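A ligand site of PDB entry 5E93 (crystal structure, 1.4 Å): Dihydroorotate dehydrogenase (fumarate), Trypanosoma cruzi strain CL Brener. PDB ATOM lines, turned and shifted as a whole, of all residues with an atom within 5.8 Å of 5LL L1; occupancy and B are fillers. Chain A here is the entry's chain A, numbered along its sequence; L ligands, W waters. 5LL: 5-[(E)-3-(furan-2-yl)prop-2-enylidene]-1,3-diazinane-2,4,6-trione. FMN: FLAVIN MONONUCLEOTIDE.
The backbone NH of Gly 72 lies within hydrogen-bond range of an oxygen (O4) of 5LL L1 (3.2 Å). ND2 of Asn 129 is in hydrogen-bond range of O2 of FMN L2 (3.2 Å). O4 of FMN L2 is in hydrogen-bond range of N of Ser 46, 3.3 Å away. The side-chain hydroxyl of Ser 197 lies within hydrogen-bond range of an oxygen (O2) of 5LL L1 (2.6 Å). N3 of FMN L2 is in hydrogen-bond range of OG of Ser 46, 2.8 Å away. The side-chain amide oxygen (OD1) of Asn 69 sits at hydrogen-bond distance from a nitrogen (N3) of 5LL L1, 2.9 Å away. The side-chain amide oxygen (OD1) of Asn 196 sits at hydrogen-bond distance from a nitrogen (N1) of 5LL L1. The side-chain amide nitrogen (ND2) of Asn 129 lies within hydrogen-bond range of an oxygen (O6) of 5LL L1 (3.1 Å). The side-chain amide nitrogen of Asn 134 sits at hydrogen-bond distance from an oxygen (O4) of 5LL L1 (3.1 Å). CAH of 5LL L1 is covalently linked to SG of Cys 132 (1.9 Å). An oxygen (O4) of FMN L2 is in hydrogen-bond range of the side-chain amino group of Lys 45 (2.7 Å).
N1 of 5LL L1 sits close to N1 of FMN L2, 3.4 Å away.
The side-chain amide oxygen of Asn 129 sits at hydrogen-bond distance from the backbone NH of Cys 132, 3.4 Å away. The side-chain sulfur (SG) of Cys 132 lies close to the backbone NH (N) of Asn 134 (3.6 Å). The backbone NH (N) of Met 71 lies within hydrogen-bond range of the side-chain amide oxygen (OD1) of Asn 69 (3.1 Å). OD1 of Asn 129 is in hydrogen-bond range of N of Ser 131. The backbone carbonyl oxygen of Cys 47 is in hydrogen-bond range of the backbone NH of Ser 101 (2.9 Å). OG1 of Thr 48 lies within hydrogen-bond range of ND2 of Asn 75, 3.2 Å away. The side-chain amide nitrogen (ND2) of Asn 196 is in hydrogen-bond range of the side-chain amide oxygen (OD1) of Asn 129 (3.4 Å). The backbone NH (N) of Asn 129 is in hydrogen-bond range of the backbone carbonyl oxygen (O) of Ile 100 (2.9 Å).
Residues that only touch 5LL L1: Leu 73 (3.0 Å), Ser 46 (3.1 Å), Ser 101 (3.1 Å), Asn 75 (3.5 Å), Pro 133 (3.6 Å), Met 71 (3.7 Å), Cys 47 (3.7 Å) and Thr 48 (3.7 Å). Within 4 Å of 5LL L1: Ser 46, Cys 47, Thr 48, Asn 69, Met 71, Gly 72, Leu 73, Asn 75, Ser 101, Asn 129, Cys 132, Pro 133, Asn 134, Asn 196 and Ser 197.
Water W1 lies within hydrogen-bond range of an oxygen (O4) of 5LL L1 (2.6 Å), the side-chain amino group of Lys 45 (2.7 Å) and the backbone carbonyl oxygen of Gly 72 (2.8 Å). Water W2 lies within hydrogen-bond range of SG of Cys 132, OG of Ser 101 and OAD of 5LL L1.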
ATOM      1  N   LYS A  45      -4.356  -5.108  30.081  1.00  0.00           N
ATOM      2  CA  LYS A  45      -3.372  -4.026  29.988  1.00  0.00           C
ATOM      3  C   LYS A  45      -1.951  -4.525  30.252  1.00  0.00           C
ATOM      4  O   LYS A  45      -1.760  -5.307  31.220  1.00  0.00           O
ATOM      5  CB  LYS A  45      -3.752  -2.999  31.088  1.00  0.00           C
ATOM      6  CG  LYS A  45      -2.689  -1.942  31.413  1.00  0.00           C
ATOM      7  CD  LYS A  45      -2.537  -1.032  30.260  1.00  0.00           C
ATOM      8  CE  LYS A  45      -1.287  -0.098  30.462  1.00  0.00           C
ATOM      9  NZ  LYS A  45      -1.170   0.750  29.141  1.00  0.00           N
ATOM     10  N   SER A  46      -0.995  -4.069  29.473  1.00  0.00           N
ATOM     11  CA  SER A  46       0.419  -4.485  29.738  1.00  0.00           C
ATOM     12  C   SER A  46       0.796  -4.131  31.171  1.00  0.00           C
ATOM     13  O   SER A  46       0.568  -3.021  31.655  1.00  0.00           O
ATOM     14  CB  SER A  46       1.436  -3.810  28.808  1.00  0.00           C
ATOM     15  OG  SER A  46       1.195  -4.294  27.494  1.00  0.00           O
ATOM     16  N   CYS A  47       1.412  -5.088  31.864  1.00  0.00           N
ATOM     17  CA  CYS A  47       1.771  -4.896  33.287  1.00  0.00           C
ATOM     18  C   CYS A  47       3.232  -5.036  33.521  1.00  0.00           C
ATOM     19  O   CYS A  47       3.981  -5.686  32.805  1.00  0.00           O
ATOM     20  CB  CYS A  47       0.955  -5.867  34.123  1.00  0.00           C
ATOM     21  SG  CYS A  47       1.223  -7.568  33.915  1.00  0.00           S
ATOM     22  N   THR A  48       3.667  -4.386  34.630  1.00  0.00           N
ATOM     23  CA  THR A  48       4.982  -4.580  35.227  1.00  0.00           C
ATOM     24  C   THR A  48       4.780  -5.401  36.437  1.00  0.00           C
ATOM     25  O   THR A  48       3.685  -5.607  36.968  1.00  0.00           O
ATOM     26  CB  THR A  48       5.612  -3.222  35.500  1.00  0.00           C
ATOM     27  OG1 THR A  48       4.712  -2.430  36.278  1.00  0.00           O
ATOM     28  CG2 THR A  48       5.926  -2.455  34.234  1.00  0.00           C
ATOM     29  N   ASN A  69      -0.761   8.985  22.238  1.00  0.00           N
ATOM     30  CA  ASN A  69      -0.728   8.653  23.666  1.00  0.00           C
ATOM     31  C   ASN A  69       0.692   8.473  24.181  1.00  0.00           C
ATOM     32  O   ASN A  69       1.552   7.951  23.484  1.00  0.00           O
ATOM     33  CB  ASN A  69      -1.545   7.368  24.032  1.00  0.00           C
ATOM     34  CG  ASN A  69      -0.783   6.061  23.902  1.00  0.00           C
ATOM     35  OD1 ASN A  69      -0.019   5.706  24.828  1.00  0.00           O
ATOM     36  ND2 ASN A  69      -0.881   5.367  22.808  1.00  0.00           N
ATOM     37  N   SER A  70       0.892   8.868  25.436  1.00  0.00           N
ATOM     38  CA  SER A  70       2.103   8.578  26.183  1.00  0.00           C
ATOM     39  C   SER A  70       1.737   8.007  27.533  1.00  0.00           C
ATOM     40  O   SER A  70       2.053   8.612  28.532  1.00  0.00           O
ATOM     41  CB  SER A  70       2.905   9.854  26.332  1.00  0.00           C
ATOM     42  OG  SER A  70       2.073  10.881  26.864  1.00  0.00           O
ATOM     43  N   MET A  71       0.960   6.931  27.531  1.00  0.00           N
ATOM     44  CA  MET A  71       0.469   6.426  28.819  1.00  0.00           C
ATOM     45  C   MET A  71       1.586   6.060  29.807  1.00  0.00           C
ATOM     46  O   MET A  71       1.439   6.391  30.974  1.00  0.00           O
ATOM     47  CB  MET A  71      -0.493   5.253  28.594  1.00  0.00           C
ATOM     48  CG  MET A  71      -1.699   5.417  27.771  1.00  0.00           C
ATOM     49  SD  MET A  71      -2.780   6.741  28.318  1.00  0.00           S
ATOM     50  CE  MET A  71      -3.418   5.947  29.750  1.00  0.00           C
ATOM     51  N   GLY A  72       2.584   5.391  29.284  1.00  0.00           N
ATOM     52  CA  GLY A  72       3.750   5.066  30.105  1.00  0.00           C
ATOM     53  C   GLY A  72       3.441   3.974  31.089  1.00  0.00           C
ATOM     54  O   GLY A  72       2.712   3.120  30.757  1.00  0.00           O
ATOM     55  N   LEU A  73       3.914   3.965  32.303  1.00  0.00           N
ATOM     56  CA  LEU A  73       3.652   2.739  33.065  1.00  0.00           C
ATOM     57  C   LEU A  73       2.124   2.149  33.421  1.00  0.00           C
ATOM     58  O   LEU A  73       2.080   1.018  33.884  1.00  0.00           O
ATOM     59  CB  LEU A  73       4.714   2.566  34.189  1.00  0.00           C
ATOM     60  CG  LEU A  73       6.009   3.454  34.305  1.00  0.00           C
ATOM     61  CD1 LEU A  73       6.992   2.677  35.186  1.00  0.00           C
ATOM     62  CD2 LEU A  73       6.859   3.891  33.174  1.00  0.00           C
ATOM     63  N   PRO A  74       0.901   2.778  33.105  1.00  0.00           N
ATOM     64  CA  PRO A  74       0.039   2.548  34.221  1.00  0.00           C
ATOM     65  C   PRO A  74      -0.717   1.262  34.328  1.00  0.00           C
ATOM     66  O   PRO A  74      -1.512   0.942  33.387  1.00  0.00           O
ATOM     67  CB  PRO A  74      -1.118   3.632  34.003  1.00  0.00           C
ATOM     68  CG  PRO A  74      -1.157   3.844  32.508  1.00  0.00           C
ATOM     69  CD  PRO A  74       0.192   3.422  31.950  1.00  0.00           C
ATOM     70  N   ASN A  75      -0.556   0.561  35.439  1.00  0.00           N
ATOM     71  CA  ASN A  75      -1.244  -0.680  35.546  1.00  0.00           C
ATOM     72  C   ASN A  75      -1.299  -1.029  37.017  1.00  0.00           C
ATOM     73  O   ASN A  75      -0.555  -0.528  37.777  1.00  0.00           O
ATOM     74  CB  ASN A  75      -0.463  -1.745  34.727  1.00  0.00           C
ATOM     75  CG  ASN A  75       0.879  -2.172  35.367  1.00  0.00           C
ATOM     76  OD1 ASN A  75       0.927  -3.141  35.952  1.00  0.00           O
ATOM     77  ND2 ASN A  75       1.855  -1.368  35.280  1.00  0.00           N
ATOM     78  N   ILE A 100       2.238  -8.697  29.127  1.00  0.00           N
ATOM     79  CA  ILE A 100       3.295  -8.248  30.077  1.00  0.00           C
ATOM     80  C   ILE A 100       4.298  -7.370  29.411  1.00  0.00           C
ATOM     81  O   ILE A 100       4.624  -7.561  28.197  1.00  0.00           O
ATOM     82  CB  ILE A 100       3.951  -9.383  30.773  1.00  0.00           C
ATOM     83  CG1 ILE A 100       4.935 -10.052  29.887  1.00  0.00           C
ATOM     84  CG2 ILE A 100       2.964 -10.333  31.467  1.00  0.00           C
ATOM     85  CD1 ILE A 100       5.680 -11.148  30.617  1.00  0.00           C
ATOM     86  N   SER A 101       4.820  -6.402  30.123  1.00  0.00           N
ATOM     87  CA  SER A 101       5.806  -5.506  29.606  1.00  0.00           C
ATOM     88  C   SER A 101       6.752  -5.112  30.727  1.00  0.00           C
ATOM     89  O   SER A 101       6.828  -3.969  31.092  1.00  0.00           O
ATOM     90  CB  SER A 101       5.137  -4.300  28.965  1.00  0.00           C
ATOM     91  OG  SER A 101       6.029  -3.614  28.149  1.00  0.00           O
ATOM     92  N   GLY A 102       7.564  -6.069  31.169  1.00  0.00           N
ATOM     93  CA  GLY A 102       8.599  -5.701  32.102  1.00  0.00           C
ATOM     94  C   GLY A 102       9.642  -4.757  31.489  1.00  0.00           C
ATOM     95  O   GLY A 102       9.848  -4.716  30.291  1.00  0.00           O
ATOM     96  N   ASN A 129       4.912  -7.965  25.361  1.00  0.00           N
ATOM     97  CA  ASN A 129       5.011  -6.676  24.697  1.00  0.00           C
ATOM     98  C   ASN A 129       6.485  -6.247  24.533  1.00  0.00           C
ATOM     99  O   ASN A 129       7.110  -5.901  25.527  1.00  0.00           O
ATOM    100  CB  ASN A 129       4.215  -5.659  25.525  1.00  0.00           C
ATOM    101  CG  ASN A 129       4.159  -4.276  24.891  1.00  0.00           C
ATOM    102  OD1 ASN A 129       4.781  -4.033  23.812  1.00  0.00           O
ATOM    103  ND2 ASN A 129       3.457  -3.380  25.520  1.00  0.00           N
ATOM    104  N   SER A 131       7.311  -3.689  22.430  1.00  0.00           N
ATOM    105  CA  SER A 131       7.156  -2.491  21.657  1.00  0.00           C
ATOM    106  C   SER A 131       6.607  -1.208  22.215  1.00  0.00           C
ATOM    107  O   SER A 131       6.231  -0.330  21.500  1.00  0.00           O
ATOM    108  CB  SER A 131       6.298  -2.841  20.446  1.00  0.00           C
ATOM    109  OG  SER A 131       5.187  -3.603  20.753  1.00  0.00           O
ATOM    110  N   CYS A 132       6.564  -1.128  23.492  1.00  0.00           N
ATOM    111  CA  CYS A 132       6.087   0.136  24.095  1.00  0.00           C
ATOM    112  C   CYS A 132       6.983   1.310  23.701  1.00  0.00           C
ATOM    113  O   CYS A 132       8.184   1.247  23.944  1.00  0.00           O
ATOM    114  CB  CYS A 132       6.089  -0.042  25.619  1.00  0.00           C
ATOM    115  SG  CYS A 132       5.463   1.477  26.446  1.00  0.00           S
ATOM    116  N   PRO A 133       6.434   2.390  23.156  1.00  0.00           N
ATOM    117  CA  PRO A 133       7.248   3.545  22.734  1.00  0.00           C
ATOM    118  C   PRO A 133       7.273   4.723  23.714  1.00  0.00           C
ATOM    119  O   PRO A 133       7.771   5.845  23.369  1.00  0.00           O
ATOM    120  CB  PRO A 133       6.551   3.955  21.404  1.00  0.00           C
ATOM    121  CG  PRO A 133       5.023   3.816  21.746  1.00  0.00           C
ATOM    122  CD  PRO A 133       5.016   2.555  22.696  1.00  0.00           C
ATOM    123  N   ASN A 134       6.729   4.492  24.916  1.00  0.00           N
ATOM    124  CA  ASN A 134       6.518   5.573  25.884  1.00  0.00           C
ATOM    125  C   ASN A 134       7.170   5.563  27.246  1.00  0.00           C
ATOM    126  O   ASN A 134       6.820   6.313  28.100  1.00  0.00           O
ATOM    127  CB  ASN A 134       5.028   5.756  26.090  1.00  0.00           C
ATOM    128  CG  ASN A 134       4.322   6.135  24.827  1.00  0.00           C
ATOM    129  OD1 ASN A 134       4.787   6.993  24.100  1.00  0.00           O
ATOM    130  ND2 ASN A 134       3.214   5.523  24.617  1.00  0.00           N
ATOM    131  N   VAL A 135       8.109   4.681  27.401  1.00  0.00           N
ATOM    132  CA  VAL A 135       8.934   4.648  28.658  1.00  0.00           C
ATOM    133  C   VAL A 135      10.294   5.372  28.415  1.00  0.00           C
ATOM    134  O   VAL A 135      11.110   4.849  27.712  1.00  0.00           O
ATOM    135  CB  VAL A 135       9.058   3.224  29.166  1.00  0.00           C
ATOM    136  CG1 VAL A 135       9.910   3.187  30.490  1.00  0.00           C
ATOM    137  CG2 VAL A 135       7.672   2.637  29.407  1.00  0.00           C
ATOM    138  N   ASN A 196       1.862  -2.475  17.456  1.00  0.00           N
ATOM    139  CA  ASN A 196       1.770  -1.415  18.456  1.00  0.00           C
ATOM    140  C   ASN A 196       1.721  -0.088  17.773  1.00  0.00           C
ATOM    141  O   ASN A 196       1.829   0.042  16.543  1.00  0.00           O
ATOM    142  CB  ASN A 196       2.956  -1.570  19.429  1.00  0.00           C
ATOM    143  CG  ASN A 196       2.632  -1.147  20.851  1.00  0.00           C
ATOM    144  OD1 ASN A 196       1.911  -0.165  21.067  1.00  0.00           O
ATOM    145  ND2 ASN A 196       3.125  -1.852  21.845  1.00  0.00           N
ATOM    146  N   SER A 197       1.538   0.966  18.575  1.00  0.00           N
ATOM    147  CA  SER A 197       1.511   2.351  18.059  1.00  0.00           C
ATOM    148  C   SER A 197       2.665   2.732  17.293  1.00  0.00           C
ATOM    149  O   SER A 197       3.801   2.237  17.526  1.00  0.00           O
ATOM    150  CB  SER A 197       1.665   3.276  19.225  1.00  0.00           C
ATOM    151  OG  SER A 197       0.591   3.087  20.033  1.00  0.00           O
ATOM    152  N   GLY A 221       2.802   7.741  20.979  1.00  0.00           N
ATOM    153  CA  GLY A 221       2.511   6.777  19.926  1.00  0.00           C
ATOM    154  C   GLY A 221       1.197   7.071  19.236  1.00  0.00           C
ATOM    155  O   GLY A 221       0.226   7.449  19.876  1.00  0.00           O
HETATM  156  C4  5LL L   1       2.000   2.698  25.690  1.00  0.00           C
HETATM  157  C5  5LL L   1       2.590   1.455  25.791  1.00  0.00           C
HETATM  158  C6  5LL L   1       2.415   0.638  24.589  1.00  0.00           C
HETATM  159  N1  5LL L   1       1.795   1.139  23.539  1.00  0.00           N
HETATM  160  N3  5LL L   1       1.204   3.056  24.667  1.00  0.00           N
HETATM  161  CAA 5LL L   1       3.210   0.029  31.198  1.00  0.00           C
HETATM  162  CAB 5LL L   1       3.229  -1.092  32.028  1.00  0.00           C
HETATM  163  CAC 5LL L   1       3.498  -2.148  31.197  1.00  0.00           C
HETATM  164  OAD 5LL L   1       3.605  -1.740  29.856  1.00  0.00           O
HETATM  165  CAE 5LL L   1       3.326  -0.492  29.932  1.00  0.00           C
HETATM  166  CAF 5LL L   1       3.411   0.359  28.844  1.00  0.00           C
HETATM  167  CAG 5LL L   1       3.528  -0.023  27.610  1.00  0.00           C
HETATM  168  CAH 5LL L   1       3.600   1.225  26.879  1.00  0.00           C
HETATM  169  O4  5LL L   1       2.123   3.549  26.703  1.00  0.00           O
HETATM  170  C2  5LL L   1       1.177   2.291  23.567  1.00  0.00           C
HETATM  171  O2  5LL L   1       0.663   2.841  22.594  1.00  0.00           O
HETATM  172  O6  5LL L   1       2.896  -0.527  24.544  1.00  0.00           O
HETATM  173  N1  FMN L   2      -0.230  -1.651  23.490  1.00  0.00           N
HETATM  174  C2  FMN L   2       0.233  -2.609  24.348  1.00  0.00           C
HETATM  175  O2  FMN L   2       0.738  -3.627  23.831  1.00  0.00           O
HETATM  176  N3  FMN L   2       0.103  -2.464  25.692  1.00  0.00           N
HETATM  177  C4  FMN L   2      -0.430  -1.407  26.310  1.00  0.00           C
HETATM  178  O4  FMN L   2      -0.576  -1.392  27.556  1.00  0.00           O
HETATM  179  C4A FMN L   2      -0.907  -0.392  25.480  1.00  0.00           C
HETATM  180  N5  FMN L   2      -1.521   0.673  26.023  1.00  0.00           N
HETATM  181  C5A FMN L   2      -2.221   1.537  25.173  1.00  0.00           C
HETATM  182  C6  FMN L   2      -2.992   2.563  25.682  1.00  0.00           C
HETATM  183  C7  FMN L   2      -3.756   3.402  24.901  1.00  0.00           C
HETATM  184  C7M FMN L   2      -4.595   4.478  25.513  1.00  0.00           C
HETATM  185  C8  FMN L   2      -3.709   3.253  23.473  1.00  0.00           C
HETATM  186  C8M FMN L   2      -4.440   4.177  22.534  1.00  0.00           C
HETATM  187  C9  FMN L   2      -2.904   2.256  22.973  1.00  0.00           C
HETATM  188  C9A FMN L   2      -2.153   1.367  23.753  1.00  0.00           C
HETATM  189  N10 FMN L   2      -1.379   0.337  23.225  1.00  0.00           N
HETATM  190  C10 FMN L   2      -0.802  -0.581  24.059  1.00  0.00           C
HETATM  191  C1' FMN L   2      -1.317   0.167  21.784  1.00  0.00           C
HETATM  192  C2' FMN L   2      -2.540  -0.475  21.192  1.00  0.00           C
HETATM  193  O2' FMN L   2      -2.645  -1.827  21.714  1.00  0.00           O
HETATM  194  C3' FMN L   2      -2.532  -0.604  19.683  1.00  0.00           C
HETATM  195  O3' FMN L   2      -1.366  -1.378  19.341  1.00  0.00           O
HETATM  196  C4' FMN L   2      -2.458   0.776  19.017  1.00  0.00           C
HETATM  197  O4' FMN L   2      -3.285   1.682  19.668  1.00  0.00           O
HETATM  198  C5' FMN L   2      -2.766   0.745  17.556  1.00  0.00           C
HETATM  199  O5' FMN L   2      -4.073   0.217  17.301  1.00  0.00           O
HETATM  200  P   FMN L   2      -5.259   1.312  16.901  1.00  0.00           P
HETATM  201  O1P FMN L   2      -4.899   1.936  15.590  1.00  0.00           O
HETATM  202  O2P FMN L   2      -5.298   2.297  18.047  1.00  0.00           O
HETATM  203  O3P FMN L   2      -6.502   0.432  16.864  1.00  0.00           O
HETATM  204  O   HOH W   1       1.114   2.195  28.677  1.00  0.00           O
HETATM  205  O   HOH W   2       6.118  -0.647  28.363  1.00  0.00           O
